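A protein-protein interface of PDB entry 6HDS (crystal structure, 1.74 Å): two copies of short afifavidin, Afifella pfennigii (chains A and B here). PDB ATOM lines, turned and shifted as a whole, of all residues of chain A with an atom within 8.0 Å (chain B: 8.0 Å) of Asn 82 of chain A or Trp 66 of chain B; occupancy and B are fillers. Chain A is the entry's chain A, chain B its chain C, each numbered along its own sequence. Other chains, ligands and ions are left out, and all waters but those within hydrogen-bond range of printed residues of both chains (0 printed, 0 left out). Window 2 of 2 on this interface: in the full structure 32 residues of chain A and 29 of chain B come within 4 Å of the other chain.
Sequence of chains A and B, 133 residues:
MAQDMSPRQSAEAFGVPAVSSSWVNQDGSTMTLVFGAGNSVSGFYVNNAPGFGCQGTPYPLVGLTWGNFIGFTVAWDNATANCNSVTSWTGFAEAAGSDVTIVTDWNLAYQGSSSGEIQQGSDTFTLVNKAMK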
ATOM      1  N   GLY A  53     -32.731  -9.251  14.470  1.00  0.00           N
ATOM      2  CA  GLY A  53     -33.360 -10.378  13.903  1.00  0.00           C
ATOM      3  C   GLY A  53     -32.422 -11.577  13.907  1.00  0.00           C
ATOM      4  O   GLY A  53     -31.318 -11.552  14.538  1.00  0.00           O
ATOM      5  N   CYS A  54     -32.859 -12.653  13.246  1.00  0.00           N
ATOM      6  CA  CYS A  54     -32.063 -13.910  13.061  1.00  0.00           C
ATOM      7  C   CYS A  54     -31.495 -14.449  14.385  1.00  0.00           C
ATOM      8  O   CYS A  54     -30.304 -14.781  14.471  1.00  0.00           O
ATOM      9  CB  CYS A  54     -30.937 -13.686  12.053  1.00  0.00           C
ATOM     10  SG  CYS A  54     -31.620 -13.460  10.402  1.00  0.00           S
ATOM     11  N   THR A  57     -30.888 -19.462  16.265  1.00  0.00           N
ATOM     12  CA  THR A  57     -30.515 -20.578  15.407  1.00  0.00           C
ATOM     13  C   THR A  57     -29.085 -20.367  14.935  1.00  0.00           C
ATOM     14  O   THR A  57     -28.618 -19.230  14.848  1.00  0.00           O
ATOM     15  CB  THR A  57     -31.471 -20.769  14.210  1.00  0.00           C
ATOM     16  OG1 THR A  57     -31.378 -19.639  13.338  1.00  0.00           O
ATOM     17  CG2 THR A  57     -32.909 -21.016  14.626  1.00  0.00           C
ATOM     18  N   TYR A  59     -25.821 -19.965  12.593  1.00  0.00           N
ATOM     19  CA  TYR A  59     -25.364 -19.373  11.337  1.00  0.00           C
ATOM     20  C   TYR A  59     -23.886 -19.672  11.218  1.00  0.00           C
ATOM     21  O   TYR A  59     -23.145 -19.590  12.196  1.00  0.00           O
ATOM     22  CB  TYR A  59     -25.642 -17.860  11.315  1.00  0.00           C
ATOM     23  CG  TYR A  59     -27.109 -17.557  11.205  1.00  0.00           C
ATOM     24  CD1 TYR A  59     -27.917 -17.583  12.331  1.00  0.00           C
ATOM     25  CD2 TYR A  59     -27.720 -17.316   9.982  1.00  0.00           C
ATOM     26  CE1 TYR A  59     -29.276 -17.323  12.274  1.00  0.00           C
ATOM     27  CE2 TYR A  59     -29.066 -17.045   9.913  1.00  0.00           C
ATOM     28  CZ  TYR A  59     -29.856 -17.082  11.046  1.00  0.00           C
ATOM     29  OH  TYR A  59     -31.175 -16.789  10.993  1.00  0.00           O
ATOM     30  N   THR A  73     -16.405 -13.810  10.219  1.00  0.00           N
ATOM     31  CA  THR A  73     -17.583 -13.260   9.592  1.00  0.00           C
ATOM     32  C   THR A  73     -18.773 -14.235   9.692  1.00  0.00           C
ATOM     33  O   THR A  73     -18.615 -15.463   9.516  1.00  0.00           O
ATOM     34  CB  THR A  73     -17.277 -12.885   8.148  1.00  0.00           C
ATOM     35  OG1 THR A  73     -16.268 -11.877   8.175  1.00  0.00           O
ATOM     36  CG2 THR A  73     -18.516 -12.444   7.406  1.00  0.00           C
ATOM     37  N   VAL A  74     -19.969 -13.673   9.884  1.00  0.00           N
ATOM     38  CA  VAL A  74     -21.244 -14.393   9.792  1.00  0.00           C
ATOM     39  C   VAL A  74     -22.157 -13.679   8.790  1.00  0.00           C
ATOM     40  O   VAL A  74     -22.450 -12.473   8.960  1.00  0.00           O
ATOM     41  CB  VAL A  74     -21.995 -14.494  11.129  1.00  0.00           C
ATOM     42  CG1 VAL A  74     -23.432 -14.955  10.879  1.00  0.00           C
ATOM     43  CG2 VAL A  74     -21.304 -15.373  12.117  1.00  0.00           C
ATOM     44  N   ALA A  75     -22.609 -14.415   7.777  1.00  0.00           N
ATOM     45  CA  ALA A  75     -23.693 -13.951   6.862  1.00  0.00           C
ATOM     46  C   ALA A  75     -25.057 -14.413   7.400  1.00  0.00           C
ATOM     47  O   ALA A  75     -25.276 -15.644   7.608  1.00  0.00           O
ATOM     48  CB  ALA A  75     -23.466 -14.451   5.479  1.00  0.00           C
ATOM     49  N   TRP A  76     -26.006 -13.483   7.563  1.00  0.00           N
ATOM     50  CA  TRP A  76     -27.312 -13.838   8.291  1.00  0.00           C
ATOM     51  C   TRP A  76     -28.305 -14.456   7.318  1.00  0.00           C
ATOM     52  O   TRP A  76     -29.314 -13.871   7.066  1.00  0.00           O
ATOM     53  CB  TRP A  76     -27.872 -12.625   9.046  1.00  0.00           C
ATOM     54  CG  TRP A  76     -26.874 -12.161  10.070  1.00  0.00           C
ATOM     55  CD1 TRP A  76     -26.027 -11.111   9.938  1.00  0.00           C
ATOM     56  CD2 TRP A  76     -26.509 -12.814  11.300  1.00  0.00           C
ATOM     57  NE1 TRP A  76     -25.203 -11.020  11.034  1.00  0.00           N
ATOM     58  CE2 TRP A  76     -25.469 -12.050  11.877  1.00  0.00           C
ATOM     59  CE3 TRP A  76     -26.981 -13.947  11.981  1.00  0.00           C
ATOM     60  CZ2 TRP A  76     -24.899 -12.352  13.107  1.00  0.00           C
ATOM     61  CZ3 TRP A  76     -26.391 -14.275  13.184  1.00  0.00           C
ATOM     62  CH2 TRP A  76     -25.402 -13.461  13.751  1.00  0.00           C
ATOM     63  N   ASP A  77     -27.971 -15.657   6.804  1.00  0.00           N
ATOM     64  CA  ASP A  77     -28.883 -16.460   6.063  1.00  0.00           C
ATOM     65  C   ASP A  77     -28.699 -17.909   6.502  1.00  0.00           C
ATOM     66  O   ASP A  77     -27.596 -18.403   6.593  1.00  0.00           O
ATOM     67  CB  ASP A  77     -28.655 -16.387   4.559  1.00  0.00           C
ATOM     68  CG  ASP A  77     -29.738 -17.120   3.788  1.00  0.00           C
ATOM     69  OD1 ASP A  77     -30.908 -16.640   3.762  1.00  0.00           O
ATOM     70  OD2 ASP A  77     -29.419 -18.161   3.251  1.00  0.00           O
ATOM     71  N   ASN A  78     -29.810 -18.540   6.861  1.00  0.00           N
ATOM     72  CA  ASN A  78     -29.814 -19.989   6.981  1.00  0.00           C
ATOM     73  C   ASN A  78     -31.171 -20.494   6.473  1.00  0.00           C
ATOM     74  O   ASN A  78     -31.966 -19.726   5.913  1.00  0.00           O
ATOM     75  CB  ASN A  78     -29.368 -20.378   8.396  1.00  0.00           C
ATOM     76  CG  ASN A  78     -30.375 -20.124   9.495  1.00  0.00           C
ATOM     77  OD1 ASN A  78     -31.540 -19.795   9.260  1.00  0.00           O
ATOM     78  ND2 ASN A  78     -29.913 -20.257  10.737  1.00  0.00           N
ATOM     79  N   ALA A  79     -31.445 -21.797   6.646  1.00  0.00           N
ATOM     80  CA  ALA A  79     -32.729 -22.393   6.187  1.00  0.00           C
ATOM     81  C   ALA A  79     -33.946 -21.776   6.888  1.00  0.00           C
ATOM     82  O   ALA A  79     -35.035 -21.849   6.340  1.00  0.00           O
ATOM     83  CB  ALA A  79     -32.711 -23.899   6.403  1.00  0.00           C
ATOM     84  N   THR A  80     -33.776 -21.211   8.086  1.00  0.00           N
ATOM     85  CA  THR A  80     -34.906 -20.757   8.923  1.00  0.00           C
ATOM     86  C   THR A  80     -35.212 -19.260   8.735  1.00  0.00           C
ATOM     87  O   THR A  80     -36.356 -18.867   8.871  1.00  0.00           O
ATOM     88  CB  THR A  80     -34.694 -21.076  10.404  1.00  0.00           C
ATOM     89  OG1 THR A  80     -33.851 -20.073  10.943  1.00  0.00           O
ATOM     90  CG2 THR A  80     -34.125 -22.462  10.651  1.00  0.00           C
ATOM     91  N   ALA A  81     -34.215 -18.425   8.416  1.00  0.00           N
ATOM     92  CA  ALA A  81     -34.454 -16.969   8.328  1.00  0.00           C
ATOM     93  C   ALA A  81     -33.264 -16.234   7.695  1.00  0.00           C
ATOM     94  O   ALA A  81     -32.131 -16.706   7.643  1.00  0.00           O
ATOM     95  CB  ALA A  81     -34.742 -16.394   9.697  1.00  0.00           C
ATOM     96  N   ASN A  82     -33.540 -14.994   7.310  1.00  0.00           N
ATOM     97  CA  ASN A  82     -32.616 -14.168   6.574  1.00  0.00           C
ATOM     98  C   ASN A  82     -32.829 -12.754   7.111  1.00  0.00           C
ATOM     99  O   ASN A  82     -33.986 -12.331   7.341  1.00  0.00           O
ATOM    100  CB  ASN A  82     -32.855 -14.288   5.064  1.00  0.00           C
ATOM    101  CG  ASN A  82     -31.884 -13.459   4.241  1.00  0.00           C
ATOM    102  OD1 ASN A  82     -30.974 -13.986   3.613  1.00  0.00           O
ATOM    103  ND2 ASN A  82     -32.044 -12.145   4.279  1.00  0.00           N
ATOM    104  N   CYS A  83     -31.719 -12.051   7.378  1.00  0.00           N
ATOM    105  CA  CYS A  83     -31.734 -10.650   7.794  1.00  0.00           C
ATOM    106  C   CYS A  83     -30.902  -9.755   6.846  1.00  0.00           C
ATOM    107  O   CYS A  83     -30.578  -8.614   7.243  1.00  0.00           O
ATOM    108  CB  CYS A  83     -31.197 -10.532   9.218  1.00  0.00           C
ATOM    109  SG  CYS A  83     -32.214 -11.383  10.460  1.00  0.00           S
ATOM    110  N   ASN A  84     -30.513 -10.278   5.670  1.00  0.00           N
ATOM    111  CA  ASN A  84     -29.918  -9.519   4.542  1.00  0.00           C
ATOM    112  C   ASN A  84     -28.812  -8.613   5.074  1.00  0.00           C
ATOM    113  O   ASN A  84     -28.871  -7.366   5.031  1.00  0.00           O
ATOM    114  CB  ASN A  84     -31.009  -8.818   3.711  1.00  0.00           C
ATOM    115  CG  ASN A  84     -30.466  -8.072   2.514  1.00  0.00           C
ATOM    116  OD1 ASN A  84     -29.583  -8.579   1.805  1.00  0.00           O
ATOM    117  ND2 ASN A  84     -30.994  -6.870   2.258  1.00  0.00           N
ATOM    118  N   SER A  85     -27.803  -9.259   5.674  1.00  0.00           N
ATOM    119  CA  SER A  85     -26.779  -8.555   6.348  1.00  0.00           C
ATOM    120  C   SER A  85     -25.619  -9.503   6.652  1.00  0.00           C
ATOM    121  O   SER A  85     -25.770 -10.747   6.606  1.00  0.00           O
ATOM    122  CB  SER A  85     -27.310  -7.957   7.598  1.00  0.00           C
ATOM    123  OG  SER A  85     -27.856  -8.988   8.423  1.00  0.00           O
ATOM    124  N   VAL A  86     -24.482  -8.889   6.962  1.00  0.00           N
ATOM    125  CA  VAL A  86     -23.286  -9.585   7.335  1.00  0.00           C
ATOM    126  C   VAL A  86     -22.647  -8.896   8.526  1.00  0.00           C
ATOM    127  O   VAL A  86     -22.498  -7.671   8.537  1.00  0.00           O
ATOM    128  CB  VAL A  86     -22.286  -9.624   6.170  1.00  0.00           C
ATOM    129  CG1 VAL A  86     -20.977 -10.268   6.609  1.00  0.00           C
ATOM    130  CG2 VAL A  86     -22.873 -10.298   4.935  1.00  0.00           C
ATOM    131  N   ALA A 109     -22.894  -4.897   8.250  1.00  0.00           N
ATOM    132  CA  ALA A 109     -23.363  -4.293   6.962  1.00  0.00           C
ATOM    133  C   ALA A 109     -24.801  -4.749   6.721  1.00  0.00           C
ATOM    134  O   ALA A 109     -25.090  -5.915   6.871  1.00  0.00           O
ATOM    135  CB  ALA A 109     -22.446  -4.651   5.820  1.00  0.00           C
ATOM    136  N   MET B   5     -26.163 -21.859  -3.304  1.00  0.00           N
ATOM    137  CA  MET B   5     -25.783 -20.687  -4.160  1.00  0.00           C
ATOM    138  C   MET B   5     -24.477 -20.984  -4.917  1.00  0.00           C
ATOM    139  O   MET B   5     -23.481 -21.388  -4.313  1.00  0.00           O
ATOM    140  CB  MET B   5     -25.601 -19.432  -3.299  1.00  0.00           C
ATOM    141  CG  MET B   5     -25.155 -18.205  -4.079  1.00  0.00           C
ATOM    142  SD  MET B   5     -26.464 -17.521  -5.130  1.00  0.00           S
ATOM    143  CE  MET B   5     -27.106 -16.246  -4.047  1.00  0.00           C
ATOM    144  N   SER B  10     -23.409 -15.744  -6.807  1.00  0.00           N
ATOM    145  CA  SER B  10     -22.947 -14.972  -5.651  1.00  0.00           C
ATOM    146  C   SER B  10     -22.195 -13.703  -6.106  1.00  0.00           C
ATOM    147  O   SER B  10     -22.431 -12.594  -5.608  1.00  0.00           O
ATOM    148  CB  SER B  10     -22.094 -15.839  -4.752  1.00  0.00           C
ATOM    149  OG  SER B  10     -21.911 -15.207  -3.497  1.00  0.00           O
ATOM    150  N   ALA B  13     -24.519 -11.176  -7.579  1.00  0.00           N
ATOM    151  CA  ALA B  13     -25.365 -10.605  -6.569  1.00  0.00           C
ATOM    152  C   ALA B  13     -24.563  -9.572  -5.771  1.00  0.00           C
ATOM    153  O   ALA B  13     -25.127  -8.652  -5.145  1.00  0.00           O
ATOM    154  CB  ALA B  13     -25.930 -11.698  -5.705  1.00  0.00           C
ATOM    155  N   PHE B  14     -23.239  -9.730  -5.790  1.00  0.00           N
ATOM    156  CA  PHE B  14     -22.376  -8.786  -5.125  1.00  0.00           C
ATOM    157  C   PHE B  14     -22.188  -7.550  -6.014  1.00  0.00           C
ATOM    158  O   PHE B  14     -22.049  -6.460  -5.516  1.00  0.00           O
ATOM    159  CB  PHE B  14     -21.045  -9.435  -4.744  1.00  0.00           C
ATOM    160  CG  PHE B  14     -20.175  -8.498  -3.961  1.00  0.00           C
ATOM    161  CD1 PHE B  14     -20.479  -8.222  -2.644  1.00  0.00           C
ATOM    162  CD2 PHE B  14     -19.080  -7.884  -4.544  1.00  0.00           C
ATOM    163  CE1 PHE B  14     -19.702  -7.347  -1.916  1.00  0.00           C
ATOM    164  CE2 PHE B  14     -18.282  -7.032  -3.797  1.00  0.00           C
ATOM    165  CZ  PHE B  14     -18.600  -6.757  -2.490  1.00  0.00           C
ATOM    166  N   PHE B  35     -15.414 -15.771  -5.559  1.00  0.00           N
ATOM    167  CA  PHE B  35     -16.616 -16.252  -4.987  1.00  0.00           C
ATOM    168  C   PHE B  35     -16.688 -17.763  -5.178  1.00  0.00           C
ATOM    169  O   PHE B  35     -16.565 -18.250  -6.287  1.00  0.00           O
ATOM    170  CB  PHE B  35     -17.820 -15.561  -5.621  1.00  0.00           C
ATOM    171  CG  PHE B  35     -17.884 -14.112  -5.228  1.00  0.00           C
ATOM    172  CD1 PHE B  35     -17.195 -13.152  -5.946  1.00  0.00           C
ATOM    173  CD2 PHE B  35     -18.573 -13.732  -4.093  1.00  0.00           C
ATOM    174  CE1 PHE B  35     -17.219 -11.821  -5.562  1.00  0.00           C
ATOM    175  CE2 PHE B  35     -18.624 -12.402  -3.731  1.00  0.00           C
ATOM    176  CZ  PHE B  35     -17.941 -11.451  -4.455  1.00  0.00           C
ATOM    177  N   GLY B  38     -21.713 -21.560  -1.955  1.00  0.00           N
ATOM    178  CA  GLY B  38     -22.479 -20.987  -0.908  1.00  0.00           C
ATOM    179  C   GLY B  38     -22.267 -19.483  -0.908  1.00  0.00           C
ATOM    180  O   GLY B  38     -22.437 -18.790  -1.940  1.00  0.00           O
ATOM    181  N   ASN B  39     -21.777 -19.006   0.231  1.00  0.00           N
ATOM    182  CA  ASN B  39     -21.594 -17.605   0.465  1.00  0.00           C
ATOM    183  C   ASN B  39     -20.105 -17.239   0.556  1.00  0.00           C
ATOM    184  O   ASN B  39     -19.807 -16.144   0.990  1.00  0.00           O
ATOM    185  CB  ASN B  39     -22.362 -17.239   1.735  1.00  0.00           C
ATOM    186  CG  ASN B  39     -23.855 -17.353   1.518  1.00  0.00           C
ATOM    187  OD1 ASN B  39     -24.584 -17.698   2.444  1.00  0.00           O
ATOM    188  ND2 ASN B  39     -24.302 -17.092   0.292  1.00  0.00           N
ATOM    189  N   SER B  40     -19.194 -18.116   0.109  1.00  0.00           N
ATOM    190  CA  SER B  40     -17.756 -17.987   0.469  1.00  0.00           C
ATOM    191  C   SER B  40     -17.039 -17.029  -0.477  1.00  0.00           C
ATOM    192  O   SER B  40     -17.322 -16.955  -1.679  1.00  0.00           O
ATOM    193  CB  SER B  40     -17.059 -19.326   0.505  1.00  0.00           C
ATOM    194  OG  SER B  40     -17.489 -20.104  -0.594  1.00  0.00           O
ATOM    195  N   VAL B  41     -16.098 -16.283   0.090  1.00  0.00           N
ATOM    196  CA  VAL B  41     -15.075 -15.584  -0.648  1.00  0.00           C
ATOM    197  C   VAL B  41     -13.728 -16.003  -0.094  1.00  0.00           C
ATOM    198  O   VAL B  41     -13.548 -16.172   1.072  1.00  0.00           O
ATOM    199  CB  VAL B  41     -15.169 -14.039  -0.659  1.00  0.00           C
ATOM    200  CG1 VAL B  41     -16.390 -13.552  -1.395  1.00  0.00           C
ATOM    201  CG2 VAL B  41     -15.094 -13.434   0.728  1.00  0.00           C
ATOM    202  N   LEU B  64     -17.341 -14.162   3.954  1.00  0.00           N
ATOM    203  CA  LEU B  64     -18.666 -14.515   3.401  1.00  0.00           C
ATOM    204  C   LEU B  64     -19.338 -13.296   2.806  1.00  0.00           C
ATOM    205  O   LEU B  64     -19.132 -12.188   3.301  1.00  0.00           O
ATOM    206  CB  LEU B  64     -19.554 -15.086   4.499  1.00  0.00           C
ATOM    207  CG  LEU B  64     -19.067 -16.385   5.133  1.00  0.00           C
ATOM    208  CD1 LEU B  64     -19.803 -16.666   6.424  1.00  0.00           C
ATOM    209  CD2 LEU B  64     -19.225 -17.543   4.144  1.00  0.00           C
ATOM    210  N   THR B  65     -20.223 -13.541   1.822  1.00  0.00           N
ATOM    211  CA  THR B  65     -21.087 -12.500   1.344  1.00  0.00           C
ATOM    212  C   THR B  65     -22.554 -12.920   1.421  1.00  0.00           C
ATOM    213  O   THR B  65     -22.901 -14.106   1.504  1.00  0.00           O
ATOM    214  CB  THR B  65     -20.826 -12.087  -0.105  1.00  0.00           C
ATOM    215  OG1 THR B  65     -21.220 -13.166  -0.958  1.00  0.00           O
ATOM    216  CG2 THR B  65     -19.386 -11.692  -0.338  1.00  0.00           C
ATOM    217  N   TRP B  66     -23.404 -11.898   1.427  1.00  0.00           N
ATOM    218  CA  TRP B  66     -24.795 -12.062   1.171  1.00  0.00           C
ATOM    219  C   TRP B  66     -25.286 -10.862   0.377  1.00  0.00           C
ATOM    220  O   TRP B  66     -25.230  -9.735   0.873  1.00  0.00           O
ATOM    221  CB  TRP B  66     -25.619 -12.216   2.449  1.00  0.00           C
ATOM    222  CG  TRP B  66     -27.050 -12.344   2.067  1.00  0.00           C
ATOM    223  CD1 TRP B  66     -27.993 -11.361   1.977  1.00  0.00           C
ATOM    224  CD2 TRP B  66     -27.657 -13.534   1.549  1.00  0.00           C
ATOM    225  NE1 TRP B  66     -29.160 -11.869   1.467  1.00  0.00           N
ATOM    226  CE2 TRP B  66     -28.975 -13.196   1.181  1.00  0.00           C
ATOM    227  CE3 TRP B  66     -27.191 -14.836   1.336  1.00  0.00           C
ATOM    228  CZ2 TRP B  66     -29.850 -14.146   0.664  1.00  0.00           C
ATOM    229  CZ3 TRP B  66     -28.057 -15.774   0.818  1.00  0.00           C
ATOM    230  CH2 TRP B  66     -29.367 -15.421   0.485  1.00  0.00           C
ATOM    231  N   GLY B  67     -25.811 -11.101  -0.821  1.00  0.00           N
ATOM    232  CA  GLY B  67     -26.239  -9.976  -1.558  1.00  0.00           C
ATOM    233  C   GLY B  67     -25.047  -9.068  -1.843  1.00  0.00           C
ATOM    234  O   GLY B  67     -23.997  -9.536  -2.329  1.00  0.00           O
ATOM    235  N   ASN B  68     -25.193  -7.744  -1.617  1.00  0.00           N
ATOM    236  CA  ASN B  68     -24.102  -6.846  -1.920  1.00  0.00           C
ATOM    237  C   ASN B  68     -23.285  -6.576  -0.648  1.00  0.00           C
ATOM    238  O   ASN B  68     -22.552  -5.600  -0.598  1.00  0.00           O
ATOM    239  CB  ASN B  68     -24.531  -5.492  -2.472  1.00  0.00           C
ATOM    240  CG  ASN B  68     -25.338  -4.653  -1.526  1.00  0.00           C
ATOM    241  OD1 ASN B  68     -26.259  -5.145  -0.871  1.00  0.00           O
ATOM    242  ND2 ASN B  68     -25.019  -3.369  -1.497  1.00  0.00           N
ATOM    243  N   PHE B  69     -23.551  -7.374   0.394  1.00  0.00           N
ATOM    244  CA  PHE B  69     -22.834  -7.293   1.712  1.00  0.00           C
ATOM    245  C   PHE B  69     -21.703  -8.306   1.806  1.00  0.00           C
ATOM    246  O   PHE B  69     -21.825  -9.489   1.327  1.00  0.00           O
ATOM    247  CB  PHE B  69     -23.849  -7.476   2.846  1.00  0.00           C
ATOM    248  CG  PHE B  69     -24.953  -6.462   2.816  1.00  0.00           C
ATOM    249  CD1 PHE B  69     -24.662  -5.105   2.681  1.00  0.00           C
ATOM    250  CD2 PHE B  69     -26.281  -6.846   2.821  1.00  0.00           C
ATOM    251  CE1 PHE B  69     -25.681  -4.172   2.556  1.00  0.00           C
ATOM    252  CE2 PHE B  69     -27.296  -5.909   2.716  1.00  0.00           C
ATOM    253  CZ  PHE B  69     -26.995  -4.570   2.608  1.00  0.00           C
ATOM    254  N   ILE B  70     -20.591  -7.873   2.431  1.00  0.00           N
ATOM    255  CA  ILE B  70     -19.407  -8.683   2.506  1.00  0.00           C
ATOM    256  C   ILE B  70     -18.699  -8.450   3.834  1.00  0.00           C
ATOM    257  O   ILE B  70     -18.628  -7.344   4.331  1.00  0.00           O
ATOM    258  CB  ILE B  70     -18.463  -8.409   1.332  1.00  0.00           C
ATOM    259  CG1 ILE B  70     -17.309  -9.397   1.321  1.00  0.00           C
ATOM    260  CG2 ILE B  70     -17.965  -6.964   1.297  1.00  0.00           C
ATOM    261  CD1 ILE B  70     -16.613  -9.458  -0.017  1.00  0.00           C
ATOM    262  N   GLY B  71     -18.095  -9.516   4.324  1.00  0.00           N
ATOM    263  CA  GLY B  71     -17.136  -9.471   5.434  1.00  0.00           C
ATOM    264  C   GLY B  71     -15.987 -10.405   5.140  1.00  0.00           C
ATOM    265  O   GLY B  71     -16.222 -11.461   4.628  1.00  0.00           O
ATOM    266  N   GLY B  91     -18.566  -4.551   4.703  1.00  0.00           N
ATOM    267  CA  GLY B  91     -19.122  -3.472   3.978  1.00  0.00           C
ATOM    268  C   GLY B  91     -20.127  -3.923   2.961  1.00  0.00           C
ATOM    269  O   GLY B  91     -20.709  -5.023   3.057  1.00  0.00           O
ATOM    270  N   PHE B  92     -20.322  -3.035   1.994  1.00  0.00           N
ATOM    271  CA  PHE B  92     -21.352  -3.176   0.980  1.00  0.00           C
ATOM    272  C   PHE B  92     -20.821  -2.688  -0.368  1.00  0.00           C
ATOM    273  O   PHE B  92     -20.080  -1.679  -0.430  1.00  0.00           O
ATOM    274  CB  PHE B  92     -22.596  -2.413   1.425  1.00  0.00           C
ATOM    275  CG  PHE B  92     -22.437  -0.924   1.565  1.00  0.00           C
ATOM    276  CD1 PHE B  92     -22.618  -0.072   0.481  1.00  0.00           C
ATOM    277  CD2 PHE B  92     -22.138  -0.370   2.796  1.00  0.00           C
ATOM    278  CE1 PHE B  92     -22.480   1.308   0.622  1.00  0.00           C
ATOM    279  CE2 PHE B  92     -21.972   1.001   2.927  1.00  0.00           C
ATOM    280  CZ  PHE B  92     -22.146   1.839   1.846  1.00  0.00           C
ATOM    281  N   ALA B  93     -21.282  -3.334  -1.465  1.00  0.00           N
ATOM    282  CA  ALA B  93     -20.872  -2.938  -2.822  1.00  0.00           C
ATOM    283  C   ALA B  93     -21.990  -2.110  -3.454  1.00  0.00           C
ATOM    284  O   ALA B  93     -23.154  -2.360  -3.173  1.00  0.00           O
ATOM    285  CB  ALA B  93     -20.560  -4.131  -3.693  1.00  0.00           C
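NE1 of Trp 66 of chain B lies close to OD1 of Asn 84 of chain A, 3.3 Å away.
The backbone NH (N) of Trp 76 of chain A is in hydrogen-bond range of the backbone carbonyl oxygen (O) of Ser 85 of chain A (2.9 Å). The side-chain amide oxygen (OD1) of Asn 82 of chain A lies close to the side-chain carboxylate (OD1) of Asp 77 of chain A (2.7 Å). The backbone carbonyl oxygen (O) of Cys 83 of chain A is in hydrogen-bond range of the side-chain hydroxyl (OG) of Ser 85 of chain A, 3.0 Å away. O of Val 86 of chain A sits at hydrogen-bond distance from N of Ala 109 of chain A (2.8 Å). N of Gly 91 of chain B sits at hydrogen-bond distance from O of Ile 70 of chain B, at 2.8 Å. SG of Cys 83 of chain A forms a disulfide with SG of Cys 54 of chain A (2.2 Å).
Among the printed residues, pairs that only touch across the chains: Asn 84 of chain A with Phe 69 of chain B (3.2 Å), Asn 82 of chain A with Trp 66 of chain B (3.2 Å), Ala 109 of chain A with Gly 91 of chain B (3.3 Å), Thr 73 of chain A with Gly 71 of chain B (3.4 Å), Thr 73 of chain A with Leu 64 of chain B (3.5 Å), Val 86 of chain A with Phe 69 of chain B (3.6 Å), Asp 77 of chain A with Trp 66 of chain B (3.7 Å), Val 86 of chain A with Gly 71 of chain B (3.8 Å), Ala 75 of chain A with Leu 64 of chain B (3.8 Å), Ala 109 of chain A with Phe 69 of chain B (3.9 Å), Val 86 of chain A with Trp 66 of chain B (3.9 Å) and Ser 85 of chain A with Phe 69 of chain B (3.95 Å).
Printed residues of chain B within 4 Å of Ala 75 of chain A: Leu 64. No residue of chain B comes within 4 Å of Ala 81 of chain A. Of chain B, only Trp 66 comes within 4 Å of Asn 82 of chain A. Of the printed residues of chain B, Asn 84 of chain A touches Trp 66 and Phe 69. No residue of chain A comes within 4 Å of Gly 67 of chain B. Of the printed residues of chain A, Gly 91 of chain B touches Ala 109 (3.3 Å). The nearest residue of chain A that does not touch Trp 66 of chain B is Ser 85 of chain A (4.3 Å). The nearest printed residue of chain B that does not touch Asp 77 of chain A is Asn 39 of chain B (4.8 Å).
Of the 20 printed residues of chain B, 5 touch a printed residue of chain A. Printed residues of chain B that touch a printed residue of chain A: Leu 64, Trp 66, Phe 69, Gly 71 and Gly 91. Hydrophobic or aromatic side chains of chain B within 4 Å of the printed part of chain A: Leu 64, Trp 66 and Phe 69. Hydrophobic or aromatic side chains of chain A that line the printed part of chain B: Val 86 and Ala 109. Along chain A the printed residues that touch a printed residue of chain B span positions 73 to 109. Among the printed residues, 13 pairs touch across the chains. Among the printed residues, no Asp or Glu carboxylate lies within 4 Å of a Lys or Arg side-chain nitrogen of the other chain.
No position is printed for both chains.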
